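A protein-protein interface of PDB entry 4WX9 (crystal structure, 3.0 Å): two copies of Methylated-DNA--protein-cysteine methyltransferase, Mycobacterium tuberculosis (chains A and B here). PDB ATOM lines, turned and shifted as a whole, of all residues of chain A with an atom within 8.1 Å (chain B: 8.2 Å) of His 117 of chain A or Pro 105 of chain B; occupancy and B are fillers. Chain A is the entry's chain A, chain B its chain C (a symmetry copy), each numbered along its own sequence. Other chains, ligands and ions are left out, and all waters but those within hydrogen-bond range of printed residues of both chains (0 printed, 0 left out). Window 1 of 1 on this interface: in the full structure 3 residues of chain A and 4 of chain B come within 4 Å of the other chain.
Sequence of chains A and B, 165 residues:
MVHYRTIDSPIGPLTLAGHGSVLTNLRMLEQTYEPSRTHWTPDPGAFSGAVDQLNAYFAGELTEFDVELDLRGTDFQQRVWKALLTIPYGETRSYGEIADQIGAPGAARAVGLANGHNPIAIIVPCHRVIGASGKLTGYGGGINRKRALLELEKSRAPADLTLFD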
ATOM      1  N   THR A  24      22.950  15.289 -11.777  1.00  0.00           N
ATOM      2  CA  THR A  24      22.489  16.524 -11.160  1.00  0.00           C
ATOM      3  C   THR A  24      21.155  16.329 -10.545  1.00  0.00           C
ATOM      4  O   THR A  24      20.895  16.910  -9.501  1.00  0.00           O
ATOM      5  CB  THR A  24      22.269  17.662 -12.161  1.00  0.00           C
ATOM      6  OG1 THR A  24      21.166  17.332 -13.011  1.00  0.00           O
ATOM      7  CG2 THR A  24      23.506  17.912 -12.990  1.00  0.00           C
ATOM      8  N   ASN A  25      20.289  15.582 -11.243  1.00  0.00           N
ATOM      9  CA  ASN A  25      18.919  15.307 -10.796  1.00  0.00           C
ATOM     10  C   ASN A  25      18.510  13.853 -10.890  1.00  0.00           C
ATOM     11  O   ASN A  25      19.017  13.089 -11.699  1.00  0.00           O
ATOM     12  CB  ASN A  25      17.907  16.084 -11.620  1.00  0.00           C
ATOM     13  CG  ASN A  25      18.208  17.560 -11.687  1.00  0.00           C
ATOM     14  OD1 ASN A  25      17.605  18.272 -12.473  1.00  0.00           O
ATOM     15  ND2 ASN A  25      19.132  18.029 -10.869  1.00  0.00           N
ATOM     16  N   GLN A  31       6.437  14.752  -8.566  1.00  0.00           N
ATOM     17  CA  GLN A  31       7.222  15.199  -7.408  1.00  0.00           C
ATOM     18  C   GLN A  31       7.231  16.719  -7.287  1.00  0.00           C
ATOM     19  O   GLN A  31       6.778  17.427  -8.189  1.00  0.00           O
ATOM     20  CB  GLN A  31       8.666  14.663  -7.523  1.00  0.00           C
ATOM     21  CG  GLN A  31       9.727  15.357  -6.665  1.00  0.00           C
ATOM     22  CD  GLN A  31      11.114  14.773  -6.847  1.00  0.00           C
ATOM     23  OE1 GLN A  31      11.336  13.590  -6.585  1.00  0.00           O
ATOM     24  NE2 GLN A  31      12.061  15.603  -7.290  1.00  0.00           N
ATOM     25  N   THR A  32       7.742  17.199  -6.152  1.00  0.00           N
ATOM     26  CA  THR A  32       7.934  18.625  -5.869  1.00  0.00           C
ATOM     27  C   THR A  32       9.390  19.094  -6.115  1.00  0.00           C
ATOM     28  O   THR A  32       9.652  20.211  -6.588  1.00  0.00           O
ATOM     29  CB  THR A  32       7.550  18.897  -4.398  1.00  0.00           C
ATOM     30  OG1 THR A  32       8.435  18.163  -3.548  1.00  0.00           O
ATOM     31  CG2 THR A  32       6.100  18.445  -4.104  1.00  0.00           C
ATOM     32  N   SER A  36      10.746  22.115 -14.523  1.00  0.00           N
ATOM     33  CA  SER A  36      11.709  23.023 -15.146  1.00  0.00           C
ATOM     34  C   SER A  36      12.853  22.243 -15.747  1.00  0.00           C
ATOM     35  O   SER A  36      13.937  22.177 -15.158  1.00  0.00           O
ATOM     36  CB  SER A  36      12.280  24.002 -14.121  1.00  0.00           C
ATOM     37  OG  SER A  36      11.284  24.885 -13.653  1.00  0.00           O
ATOM     38  N   LEU A  71      25.662  18.708  -6.938  1.00  0.00           N
ATOM     39  CA  LEU A  71      24.591  19.169  -6.084  1.00  0.00           C
ATOM     40  C   LEU A  71      24.552  20.657  -5.989  1.00  0.00           C
ATOM     41  O   LEU A  71      25.128  21.238  -5.088  1.00  0.00           O
ATOM     42  CB  LEU A  71      24.744  18.570  -4.704  1.00  0.00           C
ATOM     43  CG  LEU A  71      24.496  17.072  -4.704  1.00  0.00           C
ATOM     44  CD1 LEU A  71      24.728  16.548  -3.307  1.00  0.00           C
ATOM     45  CD2 LEU A  71      23.087  16.768  -5.165  1.00  0.00           C
ATOM     46  N   ARG A  72      23.860  21.265  -6.931  1.00  0.00           N
ATOM     47  CA  ARG A  72      23.727  22.713  -6.975  1.00  0.00           C
ATOM     48  C   ARG A  72      22.605  23.129  -6.020  1.00  0.00           C
ATOM     49  O   ARG A  72      21.499  22.587  -6.057  1.00  0.00           O
ATOM     50  CB  ARG A  72      23.433  23.175  -8.403  1.00  0.00           C
ATOM     51  CG  ARG A  72      22.082  22.669  -8.889  1.00  0.00           C
ATOM     52  CD  ARG A  72      21.902  22.696 -10.388  1.00  0.00           C
ATOM     53  NE  ARG A  72      20.731  21.895 -10.742  1.00  0.00           N
ATOM     54  CZ  ARG A  72      20.235  21.778 -11.969  1.00  0.00           C
ATOM     55  NH1 ARG A  72      20.794  22.415 -12.989  1.00  0.00           N
ATOM     56  NH2 ARG A  72      19.168  21.020 -12.180  1.00  0.00           N
ATOM     57  N   GLY A  73      22.904  24.096  -5.160  1.00  0.00           N
ATOM     58  CA  GLY A  73      21.932  24.602  -4.196  1.00  0.00           C
ATOM     59  C   GLY A  73      22.561  25.519  -3.169  1.00  0.00           C
ATOM     60  O   GLY A  73      23.775  25.611  -3.057  1.00  0.00           O
ATOM     61  N   THR A  74      21.727  26.178  -2.388  1.00  0.00           N
ATOM     62  CA  THR A  74      22.208  27.141  -1.399  1.00  0.00           C
ATOM     63  C   THR A  74      23.141  26.503  -0.385  1.00  0.00           C
ATOM     64  O   THR A  74      23.127  25.297  -0.197  1.00  0.00           O
ATOM     65  CB  THR A  74      21.057  27.751  -0.595  1.00  0.00           C
ATOM     66  OG1 THR A  74      20.462  26.725   0.205  1.00  0.00           O
ATOM     67  CG2 THR A  74      20.026  28.367  -1.510  1.00  0.00           C
ATOM     68  N   GLN A  77      21.523  24.341   2.036  1.00  0.00           N
ATOM     69  CA  GLN A  77      21.041  23.099   1.440  1.00  0.00           C
ATOM     70  C   GLN A  77      22.163  22.087   1.237  1.00  0.00           C
ATOM     71  O   GLN A  77      22.030  20.945   1.654  1.00  0.00           O
ATOM     72  CB  GLN A  77      20.331  23.384   0.133  1.00  0.00           C
ATOM     73  CG  GLN A  77      19.002  24.076   0.349  1.00  0.00           C
ATOM     74  CD  GLN A  77      18.486  24.790  -0.883  1.00  0.00           C
ATOM     75  OE1 GLN A  77      19.103  24.783  -1.942  1.00  0.00           O
ATOM     76  NE2 GLN A  77      17.337  25.419  -0.742  1.00  0.00           N
ATOM     77  N   VAL A  80      23.013  20.377   4.438  1.00  0.00           N
ATOM     78  CA  VAL A  80      21.974  19.438   4.805  1.00  0.00           C
ATOM     79  C   VAL A  80      22.130  18.170   4.002  1.00  0.00           C
ATOM     80  O   VAL A  80      22.235  17.075   4.546  1.00  0.00           O
ATOM     81  CB  VAL A  80      20.590  20.054   4.526  1.00  0.00           C
ATOM     82  CG1 VAL A  80      19.550  18.992   4.215  1.00  0.00           C
ATOM     83  CG2 VAL A  80      20.153  20.909   5.709  1.00  0.00           C
ATOM     84  N   TRP A  81      22.146  18.334   2.689  1.00  0.00           N
ATOM     85  CA  TRP A  81      22.167  17.206   1.768  1.00  0.00           C
ATOM     86  C   TRP A  81      23.408  16.356   2.031  1.00  0.00           C
ATOM     87  O   TRP A  81      23.346  15.134   2.174  1.00  0.00           O
ATOM     88  CB  TRP A  81      22.154  17.732   0.328  1.00  0.00           C
ATOM     89  CG  TRP A  81      20.898  18.460  -0.052  1.00  0.00           C
ATOM     90  CD1 TRP A  81      19.662  18.304   0.500  1.00  0.00           C
ATOM     91  CD2 TRP A  81      20.749  19.420  -1.092  1.00  0.00           C
ATOM     92  NE1 TRP A  81      18.752  19.116  -0.120  1.00  0.00           N
ATOM     93  CE2 TRP A  81      19.391  19.812  -1.108  1.00  0.00           C
ATOM     94  CE3 TRP A  81      21.624  19.987  -2.016  1.00  0.00           C
ATOM     95  CZ2 TRP A  81      18.886  20.752  -2.017  1.00  0.00           C
ATOM     96  CZ3 TRP A  81      21.121  20.928  -2.925  1.00  0.00           C
ATOM     97  CH2 TRP A  81      19.765  21.293  -2.919  1.00  0.00           C
ATOM     98  N   LEU A  84      22.638  14.328   4.744  1.00  0.00           N
ATOM     99  CA  LEU A  84      21.830  13.178   4.334  1.00  0.00           C
ATOM    100  C   LEU A  84      22.745  12.003   3.957  1.00  0.00           C
ATOM    101  O   LEU A  84      22.536  10.865   4.403  1.00  0.00           O
ATOM    102  CB  LEU A  84      20.870  13.506   3.173  1.00  0.00           C
ATOM    103  CG  LEU A  84      19.783  14.583   3.339  1.00  0.00           C
ATOM    104  CD1 LEU A  84      18.992  14.681   2.060  1.00  0.00           C
ATOM    105  CD2 LEU A  84      18.818  14.318   4.482  1.00  0.00           C
ATOM    106  N   ALA A 110      13.403  24.080   8.912  1.00  0.00           N
ATOM    107  CA  ALA A 110      14.162  24.477   7.743  1.00  0.00           C
ATOM    108  C   ALA A 110      14.793  23.272   7.091  1.00  0.00           C
ATOM    109  O   ALA A 110      14.802  23.186   5.862  1.00  0.00           O
ATOM    110  CB  ALA A 110      15.235  25.485   8.114  1.00  0.00           C
ATOM    111  N   VAL A 111      15.316  22.345   7.901  1.00  0.00           N
ATOM    112  CA  VAL A 111      15.867  21.098   7.353  1.00  0.00           C
ATOM    113  C   VAL A 111      14.766  20.451   6.498  1.00  0.00           C
ATOM    114  O   VAL A 111      14.983  20.138   5.326  1.00  0.00           O
ATOM    115  CB  VAL A 111      16.413  20.130   8.432  1.00  0.00           C
ATOM    116  CG1 VAL A 111      17.093  18.947   7.785  1.00  0.00           C
ATOM    117  CG2 VAL A 111      17.427  20.807   9.338  1.00  0.00           C
ATOM    118  N   GLY A 112      13.570  20.322   7.059  1.00  0.00           N
ATOM    119  CA  GLY A 112      12.373  19.961   6.285  1.00  0.00           C
ATOM    120  C   GLY A 112      12.308  20.489   4.860  1.00  0.00           C
ATOM    121  O   GLY A 112      12.031  19.750   3.928  1.00  0.00           O
ATOM    122  N   LEU A 113      12.584  21.764   4.670  1.00  0.00           N
ATOM    123  CA  LEU A 113      12.385  22.367   3.349  1.00  0.00           C
ATOM    124  C   LEU A 113      13.568  22.129   2.414  1.00  0.00           C
ATOM    125  O   LEU A 113      13.403  21.999   1.195  1.00  0.00           O
ATOM    126  CB  LEU A 113      12.114  23.863   3.499  1.00  0.00           C
ATOM    127  CG  LEU A 113      11.183  24.218   4.669  1.00  0.00           C
ATOM    128  CD1 LEU A 113      10.739  25.676   4.553  1.00  0.00           C
ATOM    129  CD2 LEU A 113       9.977  23.271   4.780  1.00  0.00           C
ATOM    130  N   ALA A 114      14.758  22.091   3.004  1.00  0.00           N
ATOM    131  CA  ALA A 114      15.987  21.806   2.282  1.00  0.00           C
ATOM    132  C   ALA A 114      15.871  20.402   1.817  1.00  0.00           C
ATOM    133  O   ALA A 114      16.138  20.075   0.662  1.00  0.00           O
ATOM    134  CB  ALA A 114      17.186  21.939   3.202  1.00  0.00           C
ATOM    135  N   ASN A 115      15.452  19.573   2.760  1.00  0.00           N
ATOM    136  CA  ASN A 115      15.070  18.225   2.480  1.00  0.00           C
ATOM    137  C   ASN A 115      14.040  18.160   1.344  1.00  0.00           C
ATOM    138  O   ASN A 115      14.207  17.413   0.403  1.00  0.00           O
ATOM    139  CB  ASN A 115      14.520  17.598   3.738  1.00  0.00           C
ATOM    140  CG  ASN A 115      14.625  16.114   3.714  1.00  0.00           C
ATOM    141  OD1 ASN A 115      14.926  15.541   2.689  1.00  0.00           O
ATOM    142  ND2 ASN A 115      14.397  15.477   4.839  1.00  0.00           N
ATOM    143  N   GLY A 116      12.989  18.961   1.413  1.00  0.00           N
ATOM    144  CA  GLY A 116      12.079  19.097   0.281  1.00  0.00           C
ATOM    145  C   GLY A 116      12.805  19.303  -1.039  1.00  0.00           C
ATOM    146  O   GLY A 116      12.530  18.606  -2.012  1.00  0.00           O
ATOM    147  N   HIS A 117      13.760  20.231  -1.062  1.00  0.00           N
ATOM    148  CA  HIS A 117      14.444  20.621  -2.306  1.00  0.00           C
ATOM    149  C   HIS A 117      15.567  19.698  -2.786  1.00  0.00           C
ATOM    150  O   HIS A 117      16.360  20.079  -3.635  1.00  0.00           O
ATOM    151  CB  HIS A 117      14.985  22.057  -2.175  1.00  0.00           C
ATOM    152  CG  HIS A 117      13.909  23.087  -2.092  1.00  0.00           C
ATOM    153  ND1 HIS A 117      12.837  23.111  -2.962  1.00  0.00           N
ATOM    154  CD2 HIS A 117      13.722  24.115  -1.234  1.00  0.00           C
ATOM    155  CE1 HIS A 117      12.036  24.109  -2.642  1.00  0.00           C
ATOM    156  NE2 HIS A 117      12.552  24.737  -1.599  1.00  0.00           N
ATOM    157  N   ASN A 118      15.651  18.495  -2.252  1.00  0.00           N
ATOM    158  CA  ASN A 118      16.627  17.540  -2.730  1.00  0.00           C
ATOM    159  C   ASN A 118      16.497  17.371  -4.223  1.00  0.00           C
ATOM    160  O   ASN A 118      15.449  16.978  -4.696  1.00  0.00           O
ATOM    161  CB  ASN A 118      16.379  16.197  -2.087  1.00  0.00           C
ATOM    162  CG  ASN A 118      17.341  15.160  -2.568  1.00  0.00           C
ATOM    163  OD1 ASN A 118      18.461  15.480  -2.985  1.00  0.00           O
ATOM    164  ND2 ASN A 118      16.915  13.906  -2.523  1.00  0.00           N
ATOM    165  N   PRO A 119      17.557  17.662  -4.981  1.00  0.00           N
ATOM    166  CA  PRO A 119      17.357  17.582  -6.416  1.00  0.00           C
ATOM    167  C   PRO A 119      17.517  16.152  -6.919  1.00  0.00           C
ATOM    168  O   PRO A 119      17.096  15.855  -8.044  1.00  0.00           O
ATOM    169  CB  PRO A 119      18.454  18.493  -6.968  1.00  0.00           C
ATOM    170  CG  PRO A 119      19.555  18.422  -5.967  1.00  0.00           C
ATOM    171  CD  PRO A 119      18.940  18.047  -4.640  1.00  0.00           C
ATOM    172  N   ILE A 120      18.091  15.286  -6.078  1.00  0.00           N
ATOM    173  CA  ILE A 120      18.438  13.916  -6.449  1.00  0.00           C
ATOM    174  C   ILE A 120      17.908  12.878  -5.470  1.00  0.00           C
ATOM    175  O   ILE A 120      18.571  12.527  -4.486  1.00  0.00           O
ATOM    176  CB  ILE A 120      19.955  13.748  -6.507  1.00  0.00           C
ATOM    177  CG1 ILE A 120      20.531  14.674  -7.568  1.00  0.00           C
ATOM    178  CG2 ILE A 120      20.314  12.305  -6.825  1.00  0.00           C
ATOM    179  CD1 ILE A 120      22.039  14.646  -7.636  1.00  0.00           C
ATOM    180  N   ALA A 121      16.728  12.351  -5.770  1.00  0.00           N
ATOM    181  CA  ALA A 121      16.044  11.442  -4.852  1.00  0.00           C
ATOM    182  C   ALA A 121      16.758  10.114  -4.669  1.00  0.00           C
ATOM    183  O   ALA A 121      17.562   9.705  -5.494  1.00  0.00           O
ATOM    184  CB  ALA A 121      14.624  11.199  -5.327  1.00  0.00           C
ATOM    185  N   CYS A 126      17.106  11.244   1.382  1.00  0.00           N
ATOM    186  CA  CYS A 126      16.286  12.246   2.034  1.00  0.00           C
ATOM    187  C   CYS A 126      15.021  11.634   2.611  1.00  0.00           C
ATOM    188  O   CYS A 126      14.396  12.180   3.499  1.00  0.00           O
ATOM    189  CB  CYS A 126      15.938  13.328   1.015  1.00  0.00           C
ATOM    190  SG  CYS A 126      14.499  12.972  -0.017  1.00  0.00           S
ATOM    191  N   GLY A 140       8.549  13.975  -1.099  1.00  0.00           N
ATOM    192  CA  GLY A 140       8.323  14.681  -2.364  1.00  0.00           C
ATOM    193  C   GLY A 140       7.389  13.956  -3.312  1.00  0.00           C
ATOM    194  O   GLY A 140       6.449  14.549  -3.864  1.00  0.00           O
ATOM    195  N   PHE B  76       6.359  37.845 -12.429  1.00  0.00           N
ATOM    196  CA  PHE B  76       5.936  36.788 -11.491  1.00  0.00           C
ATOM    197  C   PHE B  76       4.451  36.749 -11.113  1.00  0.00           C
ATOM    198  O   PHE B  76       3.801  35.698 -11.106  1.00  0.00           O
ATOM    199  CB  PHE B  76       6.720  37.032 -10.206  1.00  0.00           C
ATOM    200  CG  PHE B  76       6.647  35.925  -9.206  1.00  0.00           C
ATOM    201  CD1 PHE B  76       7.036  34.652  -9.542  1.00  0.00           C
ATOM    202  CD2 PHE B  76       6.267  36.180  -7.903  1.00  0.00           C
ATOM    203  CE1 PHE B  76       7.001  33.640  -8.607  1.00  0.00           C
ATOM    204  CE2 PHE B  76       6.237  35.172  -6.958  1.00  0.00           C
ATOM    205  CZ  PHE B  76       6.601  33.897  -7.313  1.00  0.00           C
ATOM    206  N   ARG B  79       2.465  35.262 -13.577  1.00  0.00           N
ATOM    207  CA  ARG B  79       2.642  33.818 -13.607  1.00  0.00           C
ATOM    208  C   ARG B  79       1.729  33.154 -12.587  1.00  0.00           C
ATOM    209  O   ARG B  79       1.093  32.135 -12.865  1.00  0.00           O
ATOM    210  CB  ARG B  79       4.090  33.430 -13.326  1.00  0.00           C
ATOM    211  CG  ARG B  79       5.064  33.742 -14.454  1.00  0.00           C
ATOM    212  CD  ARG B  79       6.533  33.712 -14.004  1.00  0.00           C
ATOM    213  NE  ARG B  79       7.027  32.366 -13.688  1.00  0.00           N
ATOM    214  CZ  ARG B  79       8.022  32.097 -12.831  1.00  0.00           C
ATOM    215  NH1 ARG B  79       8.661  33.068 -12.179  1.00  0.00           N
ATOM    216  NH2 ARG B  79       8.378  30.836 -12.606  1.00  0.00           N
ATOM    217  N   GLY B  96       2.784  26.534  -2.013  1.00  0.00           N
ATOM    218  CA  GLY B  96       3.941  25.974  -2.717  1.00  0.00           C
ATOM    219  C   GLY B  96       3.589  25.111  -3.916  1.00  0.00           C
ATOM    220  O   GLY B  96       4.348  25.016  -4.862  1.00  0.00           O
ATOM    221  N   GLU B  97       2.435  24.471  -3.878  1.00  0.00           N
ATOM    222  CA  GLU B  97       1.986  23.635  -4.983  1.00  0.00           C
ATOM    223  C   GLU B  97       1.935  24.478  -6.249  1.00  0.00           C
ATOM    224  O   GLU B  97       2.454  24.103  -7.290  1.00  0.00           O
ATOM    225  CB  GLU B  97       0.612  23.051  -4.628  1.00  0.00           C
ATOM    226  CG  GLU B  97       0.075  21.934  -5.516  1.00  0.00           C
ATOM    227  CD  GLU B  97      -1.108  21.202  -4.877  1.00  0.00           C
ATOM    228  OE1 GLU B  97      -1.251  21.250  -3.630  1.00  0.00           O
ATOM    229  OE2 GLU B  97      -1.902  20.572  -5.621  1.00  0.00           O
ATOM    230  N   ILE B  98       1.343  25.651  -6.120  1.00  0.00           N
ATOM    231  CA  ILE B  98       1.323  26.640  -7.194  1.00  0.00           C
ATOM    232  C   ILE B  98       2.752  27.043  -7.586  1.00  0.00           C
ATOM    233  O   ILE B  98       3.091  27.141  -8.772  1.00  0.00           O
ATOM    234  CB  ILE B  98       0.559  27.913  -6.758  1.00  0.00           C
ATOM    235  CG1 ILE B  98      -0.894  27.597  -6.415  1.00  0.00           C
ATOM    236  CG2 ILE B  98       0.614  28.984  -7.837  1.00  0.00           C
ATOM    237  CD1 ILE B  98      -1.741  27.181  -7.593  1.00  0.00           C
ATOM    238  N   ALA B  99       3.578  27.299  -6.579  1.00  0.00           N
ATOM    239  CA  ALA B  99       4.967  27.620  -6.812  1.00  0.00           C
ATOM    240  C   ALA B  99       5.595  26.613  -7.779  1.00  0.00           C
ATOM    241  O   ALA B  99       6.200  26.994  -8.790  1.00  0.00           O
ATOM    242  CB  ALA B  99       5.724  27.652  -5.498  1.00  0.00           C
ATOM    243  N   ASP B 100       5.420  25.328  -7.490  1.00  0.00           N
ATOM    244  CA  ASP B 100       5.963  24.287  -8.353  1.00  0.00           C
ATOM    245  C   ASP B 100       5.392  24.420  -9.760  1.00  0.00           C
ATOM    246  O   ASP B 100       6.118  24.422 -10.737  1.00  0.00           O
ATOM    247  CB  ASP B 100       5.695  22.902  -7.761  1.00  0.00           C
ATOM    248  CG  ASP B 100       6.614  22.586  -6.581  1.00  0.00           C
ATOM    249  OD1 ASP B 100       6.789  23.434  -5.671  1.00  0.00           O
ATOM    250  OD2 ASP B 100       7.180  21.479  -6.567  1.00  0.00           O
ATOM    251  N   GLN B 101       4.090  24.606  -9.847  1.00  0.00           N
ATOM    252  CA  GLN B 101       3.382  24.605 -11.127  1.00  0.00           C
ATOM    253  C   GLN B 101       3.776  25.747 -12.080  1.00  0.00           C
ATOM    254  O   GLN B 101       3.573  25.629 -13.274  1.00  0.00           O
ATOM    255  CB  GLN B 101       1.892  24.627 -10.819  1.00  0.00           C
ATOM    256  CG  GLN B 101       0.939  24.580 -11.984  1.00  0.00           C
ATOM    257  CD  GLN B 101      -0.476  24.840 -11.505  1.00  0.00           C
ATOM    258  OE1 GLN B 101      -1.128  25.793 -11.938  1.00  0.00           O
ATOM    259  NE2 GLN B 101      -0.946  24.006 -10.569  1.00  0.00           N
ATOM    260  N   ILE B 102       4.322  26.840 -11.553  1.00  0.00           N
ATOM    261  CA  ILE B 102       4.979  27.874 -12.384  1.00  0.00           C
ATOM    262  C   ILE B 102       6.489  27.739 -12.201  1.00  0.00           C
ATOM    263  O   ILE B 102       7.214  28.727 -12.130  1.00  0.00           O
ATOM    264  CB  ILE B 102       4.582  29.321 -12.005  1.00  0.00           C
ATOM    265  CG1 ILE B 102       4.652  29.522 -10.495  1.00  0.00           C
ATOM    266  CG2 ILE B 102       3.188  29.648 -12.492  1.00  0.00           C
ATOM    267  CD1 ILE B 102       4.908  30.946 -10.092  1.00  0.00           C
ATOM    268  N   GLY B 103       6.948  26.503 -12.076  1.00  0.00           N
ATOM    269  CA  GLY B 103       8.367  26.201 -12.054  1.00  0.00           C
ATOM    270  C   GLY B 103       9.236  27.087 -11.185  1.00  0.00           C
ATOM    271  O   GLY B 103      10.300  27.510 -11.623  1.00  0.00           O
ATOM    272  N   ALA B 104       8.808  27.369  -9.960  1.00  0.00           N
ATOM    273  CA  ALA B 104       9.650  28.119  -9.032  1.00  0.00           C
ATOM    274  C   ALA B 104       9.563  27.550  -7.624  1.00  0.00           C
ATOM    275  O   ALA B 104       9.054  28.202  -6.721  1.00  0.00           O
ATOM    276  CB  ALA B 104       9.260  29.588  -9.043  1.00  0.00           C
ATOM    277  N   PRO B 105      10.073  26.329  -7.423  1.00  0.00           N
ATOM    278  CA  PRO B 105       9.975  25.733  -6.087  1.00  0.00           C
ATOM    279  C   PRO B 105      10.662  26.588  -5.032  1.00  0.00           C
ATOM    280  O   PRO B 105      11.572  27.351  -5.354  1.00  0.00           O
ATOM    281  CB  PRO B 105      10.695  24.385  -6.231  1.00  0.00           C
ATOM    282  CG  PRO B 105      10.774  24.130  -7.700  1.00  0.00           C
ATOM    283  CD  PRO B 105      10.803  25.471  -8.368  1.00  0.00           C
ATOM    284  N   GLY B 106      10.213  26.466  -3.787  1.00  0.00           N
ATOM    285  CA  GLY B 106      10.756  27.255  -2.677  1.00  0.00           C
ATOM    286  C   GLY B 106      10.085  28.602  -2.472  1.00  0.00           C
ATOM    287  O   GLY B 106      10.208  29.200  -1.408  1.00  0.00           O
ATOM    288  N   ALA B 107       9.332  29.056  -3.475  1.00  0.00           N
ATOM    289  CA  ALA B 107       8.755  30.403  -3.499  1.00  0.00           C
ATOM    290  C   ALA B 107       7.356  30.460  -2.894  1.00  0.00           C
ATOM    291  O   ALA B 107       6.535  31.279  -3.309  1.00  0.00           O
ATOM    292  CB  ALA B 107       8.713  30.911  -4.933  1.00  0.00           C
ATOM    293  N   ALA B 108       7.083  29.609  -1.910  1.00  0.00           N
ATOM    294  CA  ALA B 108       5.751  29.534  -1.320  1.00  0.00           C
ATOM    295  C   ALA B 108       5.406  30.882  -0.721  1.00  0.00           C
ATOM    296  O   ALA B 108       4.501  31.578  -1.185  1.00  0.00           O
ATOM    297  CB  ALA B 108       5.687  28.438  -0.261  1.00  0.00           C
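Of the 27 printed residues of chain A, 3 touch a printed residue of chain B. Printed residues of chain A that touch a printed residue of chain B: Thr 32, Ser 36 and His 117. Hydrophobic or aromatic side chains of chain B within 4 Å of the printed part of chain A: Pro 105. Among the printed residues, no Asp or Glu carboxylate lies within 4 Å of a Lys or Arg side-chain nitrogen of the other chain.
Of chain B, only Pro 105 (3.7 Å) and Gly 106 (3.2 Å) come within 4 Å of His 117 of chain A. Printed residues of chain A within 4 Å of Pro 105 of chain B: His 117. No residue of chain B comes within 4 Å of Gly 116 of chain A. No residue of chain A comes within 4 Å of Ala 104 of chain B. Of the printed residues of chain A, Gly 103 of chain B touches Ser 36. Of the printed residues of chain A, Asp 100 of chain B touches Thr 32. Printed residues of chain B within 4 Å of Ser 36 of chain A: Gly 103 (3.5 Å). Printed residues of chain B within 4 Å of Thr 32 of chain A: Asp 100 (2.8 Å). The nearest residue of chain B that does not touch His 117 of chain A is Ala 107 of chain B (5.7 Å).
No position is printed for both chains.
The side-chain hydroxyl (OG) of Ser 36 of chain A lies within hydrogen-bond range of the backbone carbonyl oxygen (O) of Gly 103 of chain B (3.5 Å). OD2 of Asp 100 of chain B lies close to O of Thr 32 of chain A, at 2.8 Å.
Among the printed residues, merely in contact across the chains: His 117 of chain A with Pro 105 of chain B (3.7 Å) and His 117 of chain A with Gly 106 of chain B (3.2 Å).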
